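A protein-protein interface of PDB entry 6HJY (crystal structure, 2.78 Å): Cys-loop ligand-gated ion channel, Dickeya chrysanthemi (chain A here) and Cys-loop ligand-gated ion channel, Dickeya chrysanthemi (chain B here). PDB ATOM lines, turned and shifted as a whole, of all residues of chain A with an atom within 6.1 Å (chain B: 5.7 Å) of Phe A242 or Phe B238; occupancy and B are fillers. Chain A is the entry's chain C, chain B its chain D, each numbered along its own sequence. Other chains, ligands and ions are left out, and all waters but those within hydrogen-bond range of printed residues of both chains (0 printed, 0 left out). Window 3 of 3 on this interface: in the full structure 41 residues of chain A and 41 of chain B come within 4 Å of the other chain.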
ATOM      1  N   VAL A 237     -10.934  27.955  -4.016  1.00  0.00           N
ATOM      2  CA  VAL A 237     -11.402  26.908  -3.091  1.00  0.00           C
ATOM      3  C   VAL A 237     -11.630  25.597  -3.865  1.00  0.00           C
ATOM      4  O   VAL A 237     -11.305  24.536  -3.338  1.00  0.00           O
ATOM      5  CB  VAL A 237     -12.607  27.352  -2.207  1.00  0.00           C
ATOM      6  CG1 VAL A 237     -13.210  26.192  -1.416  1.00  0.00           C
ATOM      7  CG2 VAL A 237     -12.175  28.451  -1.248  1.00  0.00           C
ATOM      8  N   VAL A 238     -12.101  25.681  -5.131  1.00  0.00           N
ATOM      9  CA  VAL A 238     -12.295  24.529  -6.031  1.00  0.00           C
ATOM     10  C   VAL A 238     -10.904  23.986  -6.429  1.00  0.00           C
ATOM     11  O   VAL A 238     -10.698  22.769  -6.403  1.00  0.00           O
ATOM     12  CB  VAL A 238     -13.192  24.866  -7.267  1.00  0.00           C
ATOM     13  CG1 VAL A 238     -13.242  23.716  -8.274  1.00  0.00           C
ATOM     14  CG2 VAL A 238     -14.604  25.232  -6.833  1.00  0.00           C
ATOM     15  N   ALA A 239      -9.948  24.893  -6.759  1.00  0.00           N
ATOM     16  CA  ALA A 239      -8.565  24.550  -7.125  1.00  0.00           C
ATOM     17  C   ALA A 239      -7.830  23.921  -5.943  1.00  0.00           C
ATOM     18  O   ALA A 239      -7.001  23.031  -6.143  1.00  0.00           O
ATOM     19  CB  ALA A 239      -7.821  25.793  -7.596  1.00  0.00           C
ATOM     20  N   TYR A 240      -8.163  24.365  -4.713  1.00  0.00           N
ATOM     21  CA  TYR A 240      -7.599  23.843  -3.473  1.00  0.00           C
ATOM     22  C   TYR A 240      -8.243  22.511  -3.129  1.00  0.00           C
ATOM     23  O   TYR A 240      -7.558  21.633  -2.604  1.00  0.00           O
ATOM     24  CB  TYR A 240      -7.771  24.837  -2.312  1.00  0.00           C
ATOM     25  CG  TYR A 240      -6.677  24.706  -1.271  1.00  0.00           C
ATOM     26  CD1 TYR A 240      -5.524  25.483  -1.338  1.00  0.00           C
ATOM     27  CD2 TYR A 240      -6.777  23.771  -0.241  1.00  0.00           C
ATOM     28  CE1 TYR A 240      -4.503  25.347  -0.398  1.00  0.00           C
ATOM     29  CE2 TYR A 240      -5.755  23.618   0.696  1.00  0.00           C
ATOM     30  CZ  TYR A 240      -4.625  24.412   0.617  1.00  0.00           C
ATOM     31  OH  TYR A 240      -3.631  24.260   1.542  1.00  0.00           O
ATOM     32  N   ALA A 241      -9.554  22.353  -3.435  1.00  0.00           N
ATOM     33  CA  ALA A 241     -10.307  21.113  -3.219  1.00  0.00           C
ATOM     34  C   ALA A 241      -9.732  20.014  -4.099  1.00  0.00           C
ATOM     35  O   ALA A 241      -9.665  18.870  -3.654  1.00  0.00           O
ATOM     36  CB  ALA A 241     -11.779  21.319  -3.541  1.00  0.00           C
ATOM     37  N   PHE A 242      -9.277  20.365  -5.328  1.00  0.00           N
ATOM     38  CA  PHE A 242      -8.624  19.399  -6.208  1.00  0.00           C
ATOM     39  C   PHE A 242      -7.269  19.025  -5.615  1.00  0.00           C
ATOM     40  O   PHE A 242      -6.980  17.833  -5.502  1.00  0.00           O
ATOM     41  CB  PHE A 242      -8.475  19.906  -7.667  1.00  0.00           C
ATOM     42  CG  PHE A 242      -7.273  19.298  -8.367  1.00  0.00           C
ATOM     43  CD1 PHE A 242      -7.239  17.939  -8.676  1.00  0.00           C
ATOM     44  CD2 PHE A 242      -6.135  20.059  -8.616  1.00  0.00           C
ATOM     45  CE1 PHE A 242      -6.088  17.357  -9.219  1.00  0.00           C
ATOM     46  CE2 PHE A 242      -4.995  19.481  -9.185  1.00  0.00           C
ATOM     47  CZ  PHE A 242      -4.979  18.135  -9.477  1.00  0.00           C
ATOM     48  N   TYR A 243      -6.445  20.037  -5.241  1.00  0.00           N
ATOM     49  CA  TYR A 243      -5.111  19.849  -4.664  1.00  0.00           C
ATOM     50  C   TYR A 243      -5.114  18.846  -3.516  1.00  0.00           C
ATOM     51  O   TYR A 243      -4.223  17.997  -3.458  1.00  0.00           O
ATOM     52  CB  TYR A 243      -4.458  21.188  -4.251  1.00  0.00           C
ATOM     53  CG  TYR A 243      -3.149  21.031  -3.494  1.00  0.00           C
ATOM     54  CD1 TYR A 243      -2.007  20.539  -4.131  1.00  0.00           C
ATOM     55  CD2 TYR A 243      -3.053  21.345  -2.145  1.00  0.00           C
ATOM     56  CE1 TYR A 243      -0.807  20.373  -3.434  1.00  0.00           C
ATOM     57  CE2 TYR A 243      -1.857  21.190  -1.442  1.00  0.00           C
ATOM     58  CZ  TYR A 243      -0.740  20.688  -2.089  1.00  0.00           C
ATOM     59  OH  TYR A 243       0.432  20.526  -1.397  1.00  0.00           O
ATOM     60  N   THR A 244      -6.127  18.924  -2.626  1.00  0.00           N
ATOM     61  CA  THR A 244      -6.299  18.004  -1.501  1.00  0.00           C
ATOM     62  C   THR A 244      -6.635  16.612  -2.036  1.00  0.00           C
ATOM     63  O   THR A 244      -5.905  15.676  -1.744  1.00  0.00           O
ATOM     64  CB  THR A 244      -7.369  18.500  -0.514  1.00  0.00           C
ATOM     65  OG1 THR A 244      -8.630  18.592  -1.175  1.00  0.00           O
ATOM     66  CG2 THR A 244      -7.006  19.822   0.149  1.00  0.00           C
ATOM     67  N   SER A 245      -7.674  16.498  -2.890  1.00  0.00           N
ATOM     68  CA  SER A 245      -8.125  15.243  -3.511  1.00  0.00           C
ATOM     69  C   SER A 245      -6.988  14.476  -4.212  1.00  0.00           C
ATOM     70  O   SER A 245      -6.922  13.250  -4.114  1.00  0.00           O
ATOM     71  CB  SER A 245      -9.270  15.519  -4.481  1.00  0.00           C
ATOM     72  OG  SER A 245      -8.829  15.875  -5.782  1.00  0.00           O
ATOM     73  N   ASN A 246      -6.084  15.221  -4.880  1.00  0.00           N
ATOM     74  CA  ASN A 246      -4.914  14.723  -5.608  1.00  0.00           C
ATOM     75  C   ASN A 246      -3.851  14.094  -4.688  1.00  0.00           C
ATOM     76  O   ASN A 246      -3.090  13.249  -5.154  1.00  0.00           O
ATOM     77  CB  ASN A 246      -4.290  15.873  -6.417  1.00  0.00           C
ATOM     78  CG  ASN A 246      -3.353  15.464  -7.530  1.00  0.00           C
ATOM     79  OD1 ASN A 246      -2.154  15.765  -7.509  1.00  0.00           O
ATOM     80  ND2 ASN A 246      -3.886  14.812  -8.550  1.00  0.00           N
ATOM     81  N   ILE A 247      -3.774  14.528  -3.410  1.00  0.00           N
ATOM     82  CA  ILE A 247      -2.764  14.068  -2.448  1.00  0.00           C
ATOM     83  C   ILE A 247      -3.366  13.213  -1.318  1.00  0.00           C
ATOM     84  O   ILE A 247      -2.902  12.094  -1.103  1.00  0.00           O
ATOM     85  CB  ILE A 247      -1.922  15.268  -1.900  1.00  0.00           C
ATOM     86  CG1 ILE A 247      -1.386  16.200  -3.037  1.00  0.00           C
ATOM     87  CG2 ILE A 247      -0.792  14.824  -0.955  1.00  0.00           C
ATOM     88  CD1 ILE A 247      -0.628  15.511  -4.264  1.00  0.00           C
ATOM     89  N   LEU B 231      -3.675  32.574  -7.218  1.00  0.00           N
ATOM     90  CA  LEU B 231      -4.251  31.481  -8.003  1.00  0.00           C
ATOM     91  C   LEU B 231      -3.145  30.735  -8.757  1.00  0.00           C
ATOM     92  O   LEU B 231      -3.216  29.510  -8.867  1.00  0.00           O
ATOM     93  CB  LEU B 231      -5.310  32.039  -8.980  1.00  0.00           C
ATOM     94  CG  LEU B 231      -6.091  31.040  -9.862  1.00  0.00           C
ATOM     95  CD1 LEU B 231      -7.177  30.314  -9.066  1.00  0.00           C
ATOM     96  CD2 LEU B 231      -6.711  31.752 -11.046  1.00  0.00           C
ATOM     97  N   VAL B 233       0.148  30.558  -7.772  1.00  0.00           N
ATOM     98  CA  VAL B 233       0.947  29.846  -6.762  1.00  0.00           C
ATOM     99  C   VAL B 233       0.217  28.572  -6.340  1.00  0.00           C
ATOM    100  O   VAL B 233       0.870  27.541  -6.179  1.00  0.00           O
ATOM    101  CB  VAL B 233       1.398  30.748  -5.579  1.00  0.00           C
ATOM    102  CG1 VAL B 233       2.047  29.942  -4.452  1.00  0.00           C
ATOM    103  CG2 VAL B 233       2.372  31.805  -6.076  1.00  0.00           C
ATOM    104  N   VAL B 234      -1.130  28.623  -6.242  1.00  0.00           N
ATOM    105  CA  VAL B 234      -1.959  27.448  -5.946  1.00  0.00           C
ATOM    106  C   VAL B 234      -1.827  26.497  -7.154  1.00  0.00           C
ATOM    107  O   VAL B 234      -1.578  25.308  -6.950  1.00  0.00           O
ATOM    108  CB  VAL B 234      -3.440  27.805  -5.602  1.00  0.00           C
ATOM    109  CG1 VAL B 234      -4.306  26.554  -5.467  1.00  0.00           C
ATOM    110  CG2 VAL B 234      -3.523  28.628  -4.325  1.00  0.00           C
ATOM    111  N   ALA B 235      -1.896  27.048  -8.401  1.00  0.00           N
ATOM    112  CA  ALA B 235      -1.750  26.318  -9.676  1.00  0.00           C
ATOM    113  C   ALA B 235      -0.409  25.625  -9.803  1.00  0.00           C
ATOM    114  O   ALA B 235      -0.335  24.499 -10.303  1.00  0.00           O
ATOM    115  CB  ALA B 235      -1.965  27.248 -10.859  1.00  0.00           C
ATOM    116  N   TYR B 236       0.638  26.287  -9.308  1.00  0.00           N
ATOM    117  CA  TYR B 236       1.996  25.777  -9.302  1.00  0.00           C
ATOM    118  C   TYR B 236       2.165  24.750  -8.196  1.00  0.00           C
ATOM    119  O   TYR B 236       2.900  23.785  -8.388  1.00  0.00           O
ATOM    120  CB  TYR B 236       3.002  26.921  -9.149  1.00  0.00           C
ATOM    121  CG  TYR B 236       4.347  26.579  -9.745  1.00  0.00           C
ATOM    122  CD1 TYR B 236       4.612  26.811 -11.093  1.00  0.00           C
ATOM    123  CD2 TYR B 236       5.334  25.963  -8.983  1.00  0.00           C
ATOM    124  CE1 TYR B 236       5.841  26.470 -11.657  1.00  0.00           C
ATOM    125  CE2 TYR B 236       6.559  25.604  -9.539  1.00  0.00           C
ATOM    126  CZ  TYR B 236       6.808  25.864 -10.875  1.00  0.00           C
ATOM    127  OH  TYR B 236       8.016  25.519 -11.414  1.00  0.00           O
ATOM    128  N   ALA B 237       1.474  24.947  -7.049  1.00  0.00           N
ATOM    129  CA  ALA B 237       1.495  24.021  -5.917  1.00  0.00           C
ATOM    130  C   ALA B 237       0.808  22.715  -6.301  1.00  0.00           C
ATOM    131  O   ALA B 237       1.292  21.652  -5.908  1.00  0.00           O
ATOM    132  CB  ALA B 237       0.806  24.638  -4.708  1.00  0.00           C
ATOM    133  N   PHE B 238      -0.288  22.785  -7.107  1.00  0.00           N
ATOM    134  CA  PHE B 238      -0.966  21.567  -7.558  1.00  0.00           C
ATOM    135  C   PHE B 238      -0.230  20.917  -8.744  1.00  0.00           C
ATOM    136  O   PHE B 238      -0.415  19.721  -8.976  1.00  0.00           O
ATOM    137  CB  PHE B 238      -2.494  21.715  -7.794  1.00  0.00           C
ATOM    138  CG  PHE B 238      -3.124  22.711  -8.755  1.00  0.00           C
ATOM    139  CD1 PHE B 238      -3.148  22.461 -10.124  1.00  0.00           C
ATOM    140  CD2 PHE B 238      -3.897  23.762  -8.276  1.00  0.00           C
ATOM    141  CE1 PHE B 238      -3.816  23.330 -11.007  1.00  0.00           C
ATOM    142  CE2 PHE B 238      -4.565  24.631  -9.155  1.00  0.00           C
ATOM    143  CZ  PHE B 238      -4.521  24.409 -10.515  1.00  0.00           C
ATOM    144  N   TYR B 239       0.660  21.674  -9.431  1.00  0.00           N
ATOM    145  CA  TYR B 239       1.518  21.172 -10.513  1.00  0.00           C
ATOM    146  C   TYR B 239       2.642  20.333  -9.907  1.00  0.00           C
ATOM    147  O   TYR B 239       2.939  19.236 -10.384  1.00  0.00           O
ATOM    148  CB  TYR B 239       2.094  22.332 -11.359  1.00  0.00           C
ATOM    149  CG  TYR B 239       3.411  22.032 -12.058  1.00  0.00           C
ATOM    150  CD1 TYR B 239       3.462  21.177 -13.160  1.00  0.00           C
ATOM    151  CD2 TYR B 239       4.598  22.618 -11.639  1.00  0.00           C
ATOM    152  CE1 TYR B 239       4.667  20.897 -13.803  1.00  0.00           C
ATOM    153  CE2 TYR B 239       5.809  22.348 -12.277  1.00  0.00           C
ATOM    154  CZ  TYR B 239       5.836  21.488 -13.362  1.00  0.00           C
ATOM    155  OH  TYR B 239       7.018  21.216 -13.998  1.00  0.00           O
ATOM    156  N   THR B 240       3.256  20.889  -8.850  1.00  0.00           N
ATOM    157  CA  THR B 240       4.341  20.355  -8.046  1.00  0.00           C
ATOM    158  C   THR B 240       3.929  19.017  -7.410  1.00  0.00           C
ATOM    159  O   THR B 240       4.552  17.995  -7.708  1.00  0.00           O
ATOM    160  CB  THR B 240       4.793  21.460  -7.076  1.00  0.00           C
ATOM    161  OG1 THR B 240       5.553  22.431  -7.799  1.00  0.00           O
ATOM    162  CG2 THR B 240       5.596  20.946  -5.908  1.00  0.00           C
ATOM    163  N   SER B 241       2.853  19.028  -6.598  1.00  0.00           N
ATOM    164  CA  SER B 241       2.263  17.886  -5.889  1.00  0.00           C
ATOM    165  C   SER B 241       2.046  16.653  -6.775  1.00  0.00           C
ATOM    166  O   SER B 241       2.320  15.533  -6.341  1.00  0.00           O
ATOM    167  CB  SER B 241       0.937  18.303  -5.266  1.00  0.00           C
ATOM    168  OG  SER B 241      -0.095  18.476  -6.225  1.00  0.00           O
ATOM    169  N   ASN B 242       1.581  16.879  -8.025  1.00  0.00           N
ATOM    170  CA  ASN B 242       1.304  15.868  -9.054  1.00  0.00           C
ATOM    171  C   ASN B 242       2.573  15.122  -9.521  1.00  0.00           C
ATOM    172  O   ASN B 242       2.464  14.003 -10.026  1.00  0.00           O
ATOM    173  CB  ASN B 242       0.593  16.528 -10.251  1.00  0.00           C
ATOM    174  CG  ASN B 242      -0.082  15.586 -11.218  1.00  0.00           C
ATOM    175  OD1 ASN B 242      -0.844  14.693 -10.837  1.00  0.00           O
ATOM    176  ND2 ASN B 242       0.129  15.818 -12.506  1.00  0.00           N
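Among the printed residues, pairs that only touch across the chains: Tyr A243 with Ser B241, Ile A247 with Ser B241, Tyr A243 with Ala B237, Phe A242 with Phe B238, Asn A246 with Ser B241, Tyr A243 with Phe B238, Asn A246 with Asn B242 and Ala A239 with Phe B238.
Printed residues of chain A that touch a printed residue of chain B: Ala A239, Phe A242, Tyr A243, Asn A246 and Ile A247. Among the printed residues, 8 pairs touch across the chains.
The backbone carbonyl oxygen of Phe A242 lies within hydrogen-bond range of the side-chain hydroxyl of Ser A245. The side-chain hydroxyl (OG) of Ser B241 sits close to the backbone carbonyl oxygen (O) of Ala B237. The side-chain hydroxyl (OG) of Ser B241 sits at hydrogen-bond distance from the backbone carbonyl oxygen (O) of Phe B238 (3.0 Å).
Phe A242 touches one residue of chain B. Of chain A, only Ala A239, Phe A242 and Tyr A243 come within 4 Å of Phe B238. Printed residues of chain A within 4 Å of Ala B237: Tyr A243. Of the printed residues of chain B, Asn A246 touches Ser B241 (3.6 Å) and Asn B242 (3.7 Å). Ala B235 touches none of the printed residues of chain A. The nearest residue of chain B that does not touch Phe A242 is Asn B242 (5.5 Å).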
